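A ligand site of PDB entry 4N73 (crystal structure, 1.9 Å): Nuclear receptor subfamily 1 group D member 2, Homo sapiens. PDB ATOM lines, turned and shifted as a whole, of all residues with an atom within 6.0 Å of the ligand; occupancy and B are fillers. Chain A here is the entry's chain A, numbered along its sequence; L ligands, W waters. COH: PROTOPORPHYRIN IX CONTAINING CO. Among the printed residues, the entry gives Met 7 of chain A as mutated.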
ATOM      1  N   HIS A   2      16.353  32.650 -10.368  1.00  0.00           N
ATOM      2  CA  HIS A   2      16.289  31.346 -10.989  1.00  0.00           C
ATOM      3  C   HIS A   2      15.145  31.262 -11.975  1.00  0.00           C
ATOM      4  O   HIS A   2      14.325  32.200 -12.120  1.00  0.00           O
ATOM      5  CB  HIS A   2      16.141  30.257  -9.916  1.00  0.00           C
ATOM      6  CG  HIS A   2      17.257  30.251  -8.918  1.00  0.00           C
ATOM      7  ND1 HIS A   2      17.174  30.929  -7.717  1.00  0.00           N
ATOM      8  CD2 HIS A   2      18.476  29.679  -8.949  1.00  0.00           C
ATOM      9  CE1 HIS A   2      18.293  30.764  -7.045  1.00  0.00           C
ATOM     10  NE2 HIS A   2      19.108  30.010  -7.767  1.00  0.00           N
ATOM     11  N   LEU A   3      15.114  30.120 -12.639  1.00  0.00           N
ATOM     12  CA  LEU A   3      14.082  29.799 -13.611  1.00  0.00           C
ATOM     13  C   LEU A   3      13.673  28.349 -13.396  1.00  0.00           C
ATOM     14  O   LEU A   3      14.230  27.449 -14.021  1.00  0.00           O
ATOM     15  CB  LEU A   3      14.614  30.022 -15.023  1.00  0.00           C
ATOM     16  CG  LEU A   3      13.740  29.486 -16.180  1.00  0.00           C
ATOM     17  CD1 LEU A   3      12.257  29.668 -15.952  1.00  0.00           C
ATOM     18  CD2 LEU A   3      14.160  30.174 -17.464  1.00  0.00           C
ATOM     19  N   VAL A   4      12.691  28.113 -12.518  1.00  0.00           N
ATOM     20  CA  VAL A   4      12.428  26.751 -12.034  1.00  0.00           C
ATOM     21  C   VAL A   4      11.430  25.976 -12.903  1.00  0.00           C
ATOM     22  O   VAL A   4      10.659  25.158 -12.417  1.00  0.00           O
ATOM     23  CB  VAL A   4      11.936  26.746 -10.570  1.00  0.00           C
ATOM     24  CG1 VAL A   4      13.097  27.168  -9.624  1.00  0.00           C
ATOM     25  CG2 VAL A   4      10.725  27.633 -10.339  1.00  0.00           C
ATOM     26  N   CYS A   5      11.493  26.205 -14.194  1.00  0.00           N
ATOM     27  CA  CYS A   5      10.623  25.507 -15.129  1.00  0.00           C
ATOM     28  C   CYS A   5      11.435  24.458 -15.838  1.00  0.00           C
ATOM     29  O   CYS A   5      12.473  24.811 -16.432  1.00  0.00           O
ATOM     30  CB  CYS A   5      10.075  26.485 -16.141  1.00  0.00           C
ATOM     31  SG  CYS A   5       9.047  25.707 -17.360  1.00  0.00           S
ATOM     32  N   PRO A   6      10.992  23.195 -15.794  1.00  0.00           N
ATOM     33  CA  PRO A   6      11.820  22.142 -16.408  1.00  0.00           C
ATOM     34  C   PRO A   6      11.872  22.143 -17.929  1.00  0.00           C
ATOM     35  O   PRO A   6      12.542  21.284 -18.519  1.00  0.00           O
ATOM     36  CB  PRO A   6      11.174  20.854 -15.896  1.00  0.00           C
ATOM     37  CG  PRO A   6       9.845  21.202 -15.567  1.00  0.00           C
ATOM     38  CD  PRO A   6       9.874  22.600 -15.045  1.00  0.00           C
ATOM     39  N   MET A   7      11.161  23.053 -18.568  1.00  0.00           N
ATOM     40  CA  MET A   7      11.316  23.259 -20.009  1.00  0.00           C
ATOM     41  C   MET A   7      12.640  24.007 -20.291  1.00  0.00           C
ATOM     42  O   MET A   7      13.117  24.066 -21.439  1.00  0.00           O
ATOM     43  CB  MET A   7      10.102  24.051 -20.557  1.00  0.00           C
ATOM     44  CG  MET A   7       8.768  23.366 -20.396  1.00  0.00           C
ATOM     45  SD  MET A   7       8.625  21.821 -21.300  1.00  0.00           S
ATOM     46  CE  MET A   7       8.896  20.615 -19.975  1.00  0.00           C
ATOM     47  N   TRP A  23      15.221  35.092 -21.944  1.00  0.00           N
ATOM     48  CA  TRP A  23      14.029  34.528 -22.575  1.00  0.00           C
ATOM     49  C   TRP A  23      14.327  33.842 -23.901  1.00  0.00           C
ATOM     50  O   TRP A  23      13.752  32.799 -24.237  1.00  0.00           O
ATOM     51  CB  TRP A  23      12.979  35.595 -22.816  1.00  0.00           C
ATOM     52  CG  TRP A  23      11.710  34.934 -23.184  1.00  0.00           C
ATOM     53  CD1 TRP A  23      11.203  34.738 -24.438  1.00  0.00           C
ATOM     54  CD2 TRP A  23      10.805  34.307 -22.283  1.00  0.00           C
ATOM     55  NE1 TRP A  23      10.033  34.040 -24.367  1.00  0.00           N
ATOM     56  CE2 TRP A  23       9.780  33.749 -23.051  1.00  0.00           C
ATOM     57  CE3 TRP A  23      10.767  34.159 -20.898  1.00  0.00           C
ATOM     58  CZ2 TRP A  23       8.707  33.079 -22.473  1.00  0.00           C
ATOM     59  CZ3 TRP A  23       9.708  33.485 -20.333  1.00  0.00           C
ATOM     60  CH2 TRP A  23       8.688  32.950 -21.119  1.00  0.00           C
ATOM     61  N   PHE A  26      15.937  30.598 -23.142  1.00  0.00           N
ATOM     62  CA  PHE A  26      14.868  29.715 -22.688  1.00  0.00           C
ATOM     63  C   PHE A  26      14.091  29.178 -23.905  1.00  0.00           C
ATOM     64  O   PHE A  26      13.766  27.997 -23.985  1.00  0.00           O
ATOM     65  CB  PHE A  26      13.972  30.476 -21.709  1.00  0.00           C
ATOM     66  CG  PHE A  26      12.891  29.669 -21.052  1.00  0.00           C
ATOM     67  CD1 PHE A  26      13.016  28.300 -20.822  1.00  0.00           C
ATOM     68  CD2 PHE A  26      11.727  30.302 -20.630  1.00  0.00           C
ATOM     69  CE1 PHE A  26      11.990  27.573 -20.189  1.00  0.00           C
ATOM     70  CE2 PHE A  26      10.689  29.596 -20.017  1.00  0.00           C
ATOM     71  CZ  PHE A  26      10.812  28.220 -19.802  1.00  0.00           C
ATOM     72  N   PHE A  30      12.447  25.488 -25.045  1.00  0.00           N
ATOM     73  CA  PHE A  30      11.043  25.039 -25.096  1.00  0.00           C
ATOM     74  C   PHE A  30      10.427  25.039 -26.500  1.00  0.00           C
ATOM     75  O   PHE A  30       9.445  24.323 -26.717  1.00  0.00           O
ATOM     76  CB  PHE A  30      10.139  25.863 -24.130  1.00  0.00           C
ATOM     77  CG  PHE A  30       9.931  27.322 -24.494  1.00  0.00           C
ATOM     78  CD1 PHE A  30       9.196  27.691 -25.613  1.00  0.00           C
ATOM     79  CD2 PHE A  30      10.398  28.325 -23.673  1.00  0.00           C
ATOM     80  CE1 PHE A  30       8.981  29.028 -25.917  1.00  0.00           C
ATOM     81  CE2 PHE A  30      10.174  29.677 -23.975  1.00  0.00           C
ATOM     82  CZ  PHE A  30       9.474  30.021 -25.108  1.00  0.00           C
ATOM     83  N   VAL A  34       7.108  22.842 -28.229  1.00  0.00           N
ATOM     84  CA  VAL A  34       5.908  23.473 -28.742  1.00  0.00           C
ATOM     85  C   VAL A  34       5.589  23.045 -30.172  1.00  0.00           C
ATOM     86  O   VAL A  34       4.439  22.668 -30.497  1.00  0.00           O
ATOM     87  CB  VAL A  34       6.033  25.019 -28.661  1.00  0.00           C
ATOM     88  CG1 VAL A  34       4.871  25.732 -29.430  1.00  0.00           C
ATOM     89  CG2 VAL A  34       5.992  25.437 -27.228  1.00  0.00           C
ATOM     90  N   THR A  63      -1.725  23.764 -25.633  1.00  0.00           N
ATOM     91  CA  THR A  63      -0.370  23.293 -25.805  1.00  0.00           C
ATOM     92  C   THR A  63       0.208  22.940 -24.408  1.00  0.00           C
ATOM     93  O   THR A  63       0.803  21.852 -24.221  1.00  0.00           O
ATOM     94  CB  THR A  63       0.471  24.356 -26.549  1.00  0.00           C
ATOM     95  OG1 THR A  63       0.159  24.269 -27.956  1.00  0.00           O
ATOM     96  CG2 THR A  63       1.927  24.134 -26.368  1.00  0.00           C
ATOM     97  N   PHE A  64      -0.031  23.820 -23.443  1.00  0.00           N
ATOM     98  CA  PHE A  64       0.488  23.583 -22.086  1.00  0.00           C
ATOM     99  C   PHE A  64      -0.004  22.263 -21.502  1.00  0.00           C
ATOM    100  O   PHE A  64       0.765  21.505 -20.862  1.00  0.00           O
ATOM    101  CB  PHE A  64       0.092  24.677 -21.087  1.00  0.00           C
ATOM    102  CG  PHE A  64       0.448  24.290 -19.666  1.00  0.00           C
ATOM    103  CD1 PHE A  64       1.751  24.413 -19.230  1.00  0.00           C
ATOM    104  CD2 PHE A  64      -0.476  23.679 -18.851  1.00  0.00           C
ATOM    105  CE1 PHE A  64       2.125  23.996 -17.976  1.00  0.00           C
ATOM    106  CE2 PHE A  64      -0.120  23.262 -17.557  1.00  0.00           C
ATOM    107  CZ  PHE A  64       1.189  23.429 -17.128  1.00  0.00           C
ATOM    108  N   LEU A  67       1.586  19.277 -23.273  1.00  0.00           N
ATOM    109  CA  LEU A  67       2.952  19.133 -22.775  1.00  0.00           C
ATOM    110  C   LEU A  67       3.031  18.633 -21.319  1.00  0.00           C
ATOM    111  O   LEU A  67       3.979  17.885 -20.971  1.00  0.00           O
ATOM    112  CB  LEU A  67       3.660  20.497 -22.878  1.00  0.00           C
ATOM    113  CG  LEU A  67       4.000  20.887 -24.326  1.00  0.00           C
ATOM    114  CD1 LEU A  67       4.767  22.185 -24.359  1.00  0.00           C
ATOM    115  CD2 LEU A  67       4.792  19.781 -25.038  1.00  0.00           C
ATOM    116  N   MET A  68       2.101  19.066 -20.472  1.00  0.00           N
ATOM    117  CA  MET A  68       2.031  18.579 -19.062  1.00  0.00           C
ATOM    118  C   MET A  68       1.787  17.062 -19.009  1.00  0.00           C
ATOM    119  O   MET A  68       2.331  16.370 -18.121  1.00  0.00           O
ATOM    120  CB  MET A  68       0.917  19.320 -18.300  1.00  0.00           C
ATOM    121  CG  MET A  68       0.753  18.940 -16.814  1.00  0.00           C
ATOM    122  SD  MET A  68       2.155  19.536 -15.841  1.00  0.00           S
ATOM    123  CE  MET A  68       2.894  17.987 -15.337  1.00  0.00           C
ATOM    124  N   PHE A  71       5.077  15.338 -20.656  1.00  0.00           N
ATOM    125  CA  PHE A  71       6.249  15.452 -19.769  1.00  0.00           C
ATOM    126  C   PHE A  71       5.986  15.161 -18.268  1.00  0.00           C
ATOM    127  O   PHE A  71       6.823  15.488 -17.421  1.00  0.00           O
ATOM    128  CB  PHE A  71       6.843  16.854 -19.903  1.00  0.00           C
ATOM    129  CG  PHE A  71       7.558  17.093 -21.211  1.00  0.00           C
ATOM    130  CD1 PHE A  71       8.538  16.225 -21.655  1.00  0.00           C
ATOM    131  CD2 PHE A  71       7.246  18.192 -21.987  1.00  0.00           C
ATOM    132  CE1 PHE A  71       9.186  16.436 -22.845  1.00  0.00           C
ATOM    133  CE2 PHE A  71       7.901  18.402 -23.184  1.00  0.00           C
ATOM    134  CZ  PHE A  71       8.878  17.530 -23.600  1.00  0.00           C
ATOM    135  N   ALA A  72       4.830  14.584 -17.946  1.00  0.00           N
ATOM    136  CA  ALA A  72       4.564  14.090 -16.598  1.00  0.00           C
ATOM    137  C   ALA A  72       5.716  13.217 -16.063  1.00  0.00           C
ATOM    138  O   ALA A  72       6.074  13.309 -14.894  1.00  0.00           O
ATOM    139  CB  ALA A  72       3.258  13.299 -16.587  1.00  0.00           C
ATOM    140  N   LEU A  74       8.777  13.598 -16.266  1.00  0.00           N
ATOM    141  CA  LEU A  74       9.941  14.360 -15.817  1.00  0.00           C
ATOM    142  C   LEU A  74       9.915  14.493 -14.295  1.00  0.00           C
ATOM    143  O   LEU A  74      10.940  14.777 -13.668  1.00  0.00           O
ATOM    144  CB  LEU A  74       9.988  15.744 -16.455  1.00  0.00           C
ATOM    145  CG  LEU A  74      10.219  15.885 -17.976  1.00  0.00           C
ATOM    146  CD1 LEU A  74      10.197  17.351 -18.365  1.00  0.00           C
ATOM    147  CD2 LEU A  74      11.503  15.233 -18.471  1.00  0.00           C
ATOM    148  N   PHE A  75       8.729  14.271 -13.722  1.00  0.00           N
ATOM    149  CA  PHE A  75       8.472  14.355 -12.301  1.00  0.00           C
ATOM    150  C   PHE A  75       8.510  12.944 -11.728  1.00  0.00           C
ATOM    151  O   PHE A  75       7.667  12.095 -12.055  1.00  0.00           O
ATOM    152  CB  PHE A  75       7.111  15.035 -12.034  1.00  0.00           C
ATOM    153  CG  PHE A  75       7.018  16.434 -12.587  1.00  0.00           C
ATOM    154  CD1 PHE A  75       7.300  17.541 -11.788  1.00  0.00           C
ATOM    155  CD2 PHE A  75       6.644  16.650 -13.899  1.00  0.00           C
ATOM    156  CE1 PHE A  75       7.235  18.821 -12.319  1.00  0.00           C
ATOM    157  CE2 PHE A  75       6.582  17.919 -14.439  1.00  0.00           C
ATOM    158  CZ  PHE A  75       6.879  19.009 -13.647  1.00  0.00           C
ATOM    159  N   MET A  98      14.945  27.566  -4.625  1.00  0.00           N
ATOM    160  CA  MET A  98      15.020  28.517  -5.735  1.00  0.00           C
ATOM    161  C   MET A  98      13.690  29.186  -6.129  1.00  0.00           C
ATOM    162  O   MET A  98      13.616  29.824  -7.181  1.00  0.00           O
ATOM    163  CB  MET A  98      15.580  27.846  -6.974  1.00  0.00           C
ATOM    164  CG  MET A  98      16.790  26.995  -6.731  1.00  0.00           C
ATOM    165  SD  MET A  98      17.575  26.465  -8.238  1.00  0.00           S
ATOM    166  CE  MET A  98      17.643  24.686  -8.018  1.00  0.00           C
ATOM    167  N   GLY A  99      12.652  29.022  -5.305  1.00  0.00           N
ATOM    168  CA  GLY A  99      11.352  29.638  -5.573  1.00  0.00           C
ATOM    169  C   GLY A  99      10.195  28.771  -6.073  1.00  0.00           C
ATOM    170  O   GLY A  99       9.113  29.318  -6.338  1.00  0.00           O
ATOM    171  N   ALA A 100      10.371  27.462  -6.245  1.00  0.00           N
ATOM    172  CA  ALA A 100       9.201  26.651  -6.608  1.00  0.00           C
ATOM    173  C   ALA A 100       8.323  26.586  -5.382  1.00  0.00           C
ATOM    174  O   ALA A 100       8.797  26.875  -4.285  1.00  0.00           O
ATOM    175  CB  ALA A 100       9.580  25.287  -7.087  1.00  0.00           C
ATOM    176  N   GLY A 101       7.061  26.220  -5.561  1.00  0.00           N
ATOM    177  CA  GLY A 101       6.115  26.212  -4.458  1.00  0.00           C
ATOM    178  C   GLY A 101       4.951  25.266  -4.667  1.00  0.00           C
ATOM    179  O   GLY A 101       5.135  24.112  -5.061  1.00  0.00           O
ATOM    180  N   ASP A 102       3.751  25.758  -4.408  1.00  0.00           N
ATOM    181  CA  ASP A 102       2.564  24.929  -4.480  1.00  0.00           C
ATOM    182  C   ASP A 102       2.345  24.320  -5.867  1.00  0.00           C
ATOM    183  O   ASP A 102       1.962  23.149  -5.968  1.00  0.00           O
ATOM    184  CB  ASP A 102       1.336  25.719  -4.072  1.00  0.00           C
ATOM    185  CG  ASP A 102       1.289  25.954  -2.559  1.00  0.00           C
ATOM    186  OD1 ASP A 102       1.692  25.053  -1.806  1.00  0.00           O
ATOM    187  OD2 ASP A 102       0.841  27.038  -2.145  1.00  0.00           O
ATOM    188  N   LEU A 103       2.605  25.075  -6.939  1.00  0.00           N
ATOM    189  CA  LEU A 103       2.334  24.547  -8.270  1.00  0.00           C
ATOM    190  C   LEU A 103       3.204  23.306  -8.568  1.00  0.00           C
ATOM    191  O   LEU A 103       2.686  22.268  -9.055  1.00  0.00           O
ATOM    192  CB  LEU A 103       2.523  25.640  -9.344  1.00  0.00           C
ATOM    193  CG  LEU A 103       2.484  25.171 -10.788  1.00  0.00           C
ATOM    194  CD1 LEU A 103       1.169  24.425 -11.074  1.00  0.00           C
ATOM    195  CD2 LEU A 103       2.628  26.363 -11.745  1.00  0.00           C
ATOM    196  N   LEU A 104       4.510  23.374  -8.247  1.00  0.00           N
ATOM    197  CA  LEU A 104       5.363  22.166  -8.391  1.00  0.00           C
ATOM    198  C   LEU A 104       4.780  20.968  -7.642  1.00  0.00           C
ATOM    199  O   LEU A 104       4.700  19.854  -8.171  1.00  0.00           O
ATOM    200  CB  LEU A 104       6.812  22.429  -7.930  1.00  0.00           C
ATOM    201  CG  LEU A 104       7.788  21.248  -8.054  1.00  0.00           C
ATOM    202  CD1 LEU A 104       7.843  20.670  -9.452  1.00  0.00           C
ATOM    203  CD2 LEU A 104       9.203  21.638  -7.578  1.00  0.00           C
ATOM    204  N   ASN A 105       4.326  21.194  -6.405  1.00  0.00           N
ATOM    205  CA  ASN A 105       3.744  20.097  -5.655  1.00  0.00           C
ATOM    206  C   ASN A 105       2.522  19.482  -6.349  1.00  0.00           C
ATOM    207  O   ASN A 105       2.414  18.274  -6.471  1.00  0.00           O
ATOM    208  CB  ASN A 105       3.384  20.569  -4.240  1.00  0.00           C
ATOM    209  CG  ASN A 105       4.595  21.074  -3.478  1.00  0.00           C
ATOM    210  OD1 ASN A 105       5.730  20.658  -3.741  1.00  0.00           O
ATOM    211  ND2 ASN A 105       4.361  21.963  -2.511  1.00  0.00           N
ATOM    212  N   MET A 107       1.936  19.497  -9.455  1.00  0.00           N
ATOM    213  CA  MET A 107       2.431  18.797 -10.620  1.00  0.00           C
ATOM    214  C   MET A 107       2.962  17.439 -10.236  1.00  0.00           C
ATOM    215  O   MET A 107       2.739  16.479 -10.955  1.00  0.00           O
ATOM    216  CB  MET A 107       3.493  19.605 -11.345  1.00  0.00           C
ATOM    217  CG  MET A 107       2.913  20.771 -12.102  1.00  0.00           C
ATOM    218  SD  MET A 107       4.151  21.554 -13.111  1.00  0.00           S
ATOM    219  CE  MET A 107       3.091  22.735 -14.035  1.00  0.00           C
ATOM    220  N   HIS A 189      -0.127  27.892 -13.561  1.00  0.00           N
ATOM    221  CA  HIS A 189       1.105  28.046 -14.289  1.00  0.00           C
ATOM    222  C   HIS A 189       1.166  29.358 -15.102  1.00  0.00           C
ATOM    223  O   HIS A 189       2.232  29.979 -15.263  1.00  0.00           O
ATOM    224  CB  HIS A 189       1.258  26.880 -15.200  1.00  0.00           C
ATOM    225  CG  HIS A 189       2.460  26.959 -16.044  1.00  0.00           C
ATOM    226  ND1 HIS A 189       2.434  27.526 -17.296  1.00  0.00           N
ATOM    227  CD2 HIS A 189       3.733  26.557 -15.827  1.00  0.00           C
ATOM    228  CE1 HIS A 189       3.644  27.445 -17.824  1.00  0.00           C
ATOM    229  NE2 HIS A 189       4.440  26.883 -16.942  1.00  0.00           N
ATOM    230  N   GLU A 192       2.260  32.102 -12.875  1.00  0.00           N
ATOM    231  CA  GLU A 192       3.697  32.072 -12.654  1.00  0.00           C
ATOM    232  C   GLU A 192       4.427  32.611 -13.871  1.00  0.00           C
ATOM    233  O   GLU A 192       5.424  33.316 -13.741  1.00  0.00           O
ATOM    234  CB  GLU A 192       4.155  30.652 -12.346  1.00  0.00           C
ATOM    235  CG  GLU A 192       3.483  30.071 -11.113  1.00  0.00           C
ATOM    236  CD  GLU A 192       3.926  30.787  -9.833  1.00  0.00           C
ATOM    237  OE1 GLU A 192       5.125  31.096  -9.721  1.00  0.00           O
ATOM    238  OE2 GLU A 192       3.078  31.038  -8.945  1.00  0.00           O
ATOM    239  N   LEU A 193       3.919  32.290 -15.057  1.00  0.00           N
ATOM    240  CA  LEU A 193       4.622  32.609 -16.297  1.00  0.00           C
ATOM    241  C   LEU A 193       4.677  34.118 -16.418  1.00  0.00           C
ATOM    242  O   LEU A 193       5.735  34.698 -16.637  1.00  0.00           O
ATOM    243  CB  LEU A 193       3.934  31.996 -17.513  1.00  0.00           C
ATOM    244  CG  LEU A 193       4.692  32.028 -18.846  1.00  0.00           C
ATOM    245  CD1 LEU A 193       4.079  31.004 -19.775  1.00  0.00           C
ATOM    246  CD2 LEU A 193       4.702  33.401 -19.505  1.00  0.00           C
ATOM    247  N   LEU A 194       3.516  34.731 -16.229  1.00  0.00           N
ATOM    248  CA  LEU A 194       3.357  36.168 -16.381  1.00  0.00           C
ATOM    249  C   LEU A 194       4.035  36.976 -15.267  1.00  0.00           C
ATOM    250  O   LEU A 194       4.458  38.114 -15.476  1.00  0.00           O
ATOM    251  CB  LEU A 194       1.869  36.497 -16.464  1.00  0.00           C
ATOM    252  CG  LEU A 194       1.160  35.920 -17.699  1.00  0.00           C
ATOM    253  CD1 LEU A 194      -0.342  36.248 -17.690  1.00  0.00           C
ATOM    254  CD2 LEU A 194       1.816  36.410 -18.998  1.00  0.00           C
ATOM    255  N   PHE A 196       6.849  36.310 -14.050  1.00  0.00           N
ATOM    256  CA  PHE A 196       8.278  36.038 -14.111  1.00  0.00           C
ATOM    257  C   PHE A 196       9.158  37.263 -14.422  1.00  0.00           C
ATOM    258  O   PHE A 196       9.032  37.871 -15.479  1.00  0.00           O
ATOM    259  CB  PHE A 196       8.559  34.975 -15.156  1.00  0.00           C
ATOM    260  CG  PHE A 196      10.011  34.672 -15.333  1.00  0.00           C
ATOM    261  CD1 PHE A 196      10.668  35.032 -16.500  1.00  0.00           C
ATOM    262  CD2 PHE A 196      10.734  34.019 -14.337  1.00  0.00           C
ATOM    263  CE1 PHE A 196      12.004  34.750 -16.675  1.00  0.00           C
ATOM    264  CE2 PHE A 196      12.087  33.739 -14.509  1.00  0.00           C
ATOM    265  CZ  PHE A 196      12.731  34.106 -15.677  1.00  0.00           C
HETATM  266 CO   COH L   1       6.747  26.210 -17.023  1.00  0.00          CO
HETATM  267  CHA COH L   1       7.616  27.724 -14.007  1.00  0.00           C
HETATM  268  CHB COH L   1       7.307  29.179 -18.592  1.00  0.00           C
HETATM  269  CHC COH L   1       5.866  24.856 -19.858  1.00  0.00           C
HETATM  270  CHD COH L   1       6.276  23.362 -15.317  1.00  0.00           C
HETATM  271  NA  COH L   1       7.309  28.035 -16.413  1.00  0.00           N
HETATM  272  C1A COH L   1       7.618  28.490 -15.139  1.00  0.00           C
HETATM  273  C2A COH L   1       8.012  29.868 -15.136  1.00  0.00           C
HETATM  274  C3A COH L   1       7.919  30.293 -16.417  1.00  0.00           C
HETATM  275  C4A COH L   1       7.498  29.160 -17.209  1.00  0.00           C
HETATM  276  CMA COH L   1       8.268  31.693 -16.849  1.00  0.00           C
HETATM  277  CAA COH L   1       8.430  30.702 -13.935  1.00  0.00           C
HETATM  278  CBA COH L   1       9.861  30.410 -13.472  1.00  0.00           C
HETATM  279  CGA COH L   1      10.228  31.025 -12.124  1.00  0.00           C
HETATM  280  O1A COH L   1       9.471  31.830 -11.567  1.00  0.00           O
HETATM  281  O2A COH L   1      11.304  30.633 -11.671  1.00  0.00           O
HETATM  282  NB  COH L   1       6.619  26.867 -18.793  1.00  0.00           N
HETATM  283  C1B COH L   1       6.888  28.089 -19.319  1.00  0.00           C
HETATM  284  C2B COH L   1       6.653  28.159 -20.736  1.00  0.00           C
HETATM  285  C3B COH L   1       6.246  26.922 -21.117  1.00  0.00           C
HETATM  286  C4B COH L   1       6.214  26.152 -19.895  1.00  0.00           C
HETATM  287  CMB COH L   1       6.893  29.442 -21.495  1.00  0.00           C
HETATM  288  CAB COH L   1       5.884  26.317 -22.463  1.00  0.00           C
HETATM  289  CBB COH L   1       6.331  26.841 -23.668  1.00  0.00           C
HETATM  290  NC  COH L   1       6.197  24.513 -17.461  1.00  0.00           N
HETATM  291  C1C COH L   1       5.877  24.102 -18.701  1.00  0.00           C
HETATM  292  C2C COH L   1       5.507  22.725 -18.709  1.00  0.00           C
HETATM  293  C3C COH L   1       5.613  22.276 -17.451  1.00  0.00           C
HETATM  294  C4C COH L   1       6.043  23.408 -16.680  1.00  0.00           C
HETATM  295  CMC COH L   1       5.077  22.007 -19.958  1.00  0.00           C
HETATM  296  CAC COH L   1       5.328  20.927 -16.873  1.00  0.00           C
HETATM  297  CBC COH L   1       5.670  19.729 -17.520  1.00  0.00           C
HETATM  298  ND  COH L   1       6.894  25.654 -15.019  1.00  0.00           N
HETATM  299  C1D COH L   1       6.676  24.418 -14.539  1.00  0.00           C
HETATM  300  C2D COH L   1       6.889  24.354 -13.102  1.00  0.00           C
HETATM  301  C3D COH L   1       7.259  25.591 -12.749  1.00  0.00           C
HETATM  302  C4D COH L   1       7.258  26.408 -13.960  1.00  0.00           C
HETATM  303  CMD COH L   1       6.737  23.155 -12.198  1.00  0.00           C
HETATM  304  CAD COH L   1       7.596  26.100 -11.369  1.00  0.00           C
HETATM  305  CBD COH L   1       6.285  26.211 -10.597  1.00  0.00           C
HETATM  306  CGD COH L   1       6.480  26.614  -9.143  1.00  0.00           C
HETATM  307  O1D COH L   1       7.028  27.713  -8.960  1.00  0.00           O
HETATM  308  O2D COH L   1       6.077  25.871  -8.231  1.00  0.00           O
HETATM  309  O   HOH W   1       5.583  29.008  -6.868  1.00  0.00           O
HETATM  310  O   HOH W   2       9.120  31.088  -8.732  1.00  0.00           O
HETATM  311  O   HOH W   3      12.144  31.218  -9.322  1.00  0.00           O
HETATM  312  O   HOH W   4      11.363  33.662 -10.881  1.00  0.00           O
HETATM  313  O   HOH W   5       7.236  33.480 -11.742  1.00  0.00           O
HETATM  314  O   HOH W   6       7.352  29.720 -10.565  1.00  0.00           O
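A ring nitrogen (NE2) of His 189 binds a cobalt atom (CO) of the ligand (2.4 Å). The backbone NH (N) of Val 4 lies within hydrogen-bond range of an oxygen (O2A) of the ligand (3.0 Å). O2D of the ligand sits at hydrogen-bond distance from N of Leu 104 (2.9 Å). SG of Cys 5 binds CO of the ligand, 2.4 Å away. The backbone NH (N) of Gly 101 is in hydrogen-bond range of an oxygen (O2D) of the ligand.
ND2 of Asn 105 is in hydrogen-bond range of O of Gly 101 (3.4 Å). The side-chain sulfur (SG) of Cys 5 sits close to the backbone NH (N) of Met 7 (3.6 Å).
An oxygen (O2A) of the ligand lies close to the backbone carbonyl oxygen (O) of His 2 (3.4 Å). Leu 3 touches the ligand (CA to O2A, 3.5 Å). CD of Pro 6 touches CHD of the ligand, at 3.7 Å. CG of Met 7 touches CHC of the ligand (3.3 Å). Trp 23 touches the ligand. Phe 26 touches the ligand (CE2 to CHB, 3.7 Å). Phe 30 touches the ligand. Val 34 touches the ligand (CG2 to CBB, 3.8 Å). CE1 of Phe 64 touches C2C of the ligand, 3.7 Å away. CB of Leu 67 touches CMC of the ligand, 3.6 Å away. Met 68 touches the ligand. Phe 71 touches the ligand (CB to CBC, 3.9 Å). Phe 75 touches the ligand. Gly 99 touches the ligand. Ala 100 touches the ligand (CA to O1D, 3.4 Å). Leu 103 touches the ligand (CB to O2D, 3.7 Å). SD of Met 107 touches CMD of the ligand, at 3.2 Å. Glu 192 touches the ligand. Leu 193 touches the ligand. CB of Phe 196 touches CMA of the ligand (3.7 Å). Hydrophobic or aromatic side chains that line the ligand: Leu 3, Val 4, Pro 6, Met 7, Trp 23, Phe 26, Phe 30, Val 34, Phe 64, Leu 67, Met 68, Phe 71, Phe 75, Ala 100, Leu 103, Leu 104, Met 107, His 189, Leu 193 and Phe 196. Along chain A the residues within 4 Å of the ligand span positions 2 to 196. The nearest printed residue that does not touch the ligand is Asp 102 (4.5 Å).
Water W3 bridges an oxygen (O2A) of the ligand (2.6 Å) and the backbone carbonyl oxygen (O) of Met 98 (2.9 Å). Water W6 bridges an oxygen (O1D) of the ligand (2.6 Å) and the side-chain carboxylate (OE1) of Glu 192 (2.8 Å). Water W5 bridges the backbone carbonyl oxygen of Glu 192 (2.7 Å) and an oxygen (O1A) of the ligand (2.8 Å). Water W1 bridges O1D of the ligand (2.9 Å) and N of Gly 101 (3.4 Å). Water W2 lies within hydrogen-bond range of O1A of the ligand (3.0 Å) and O of Gly 99 (3.0 Å).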
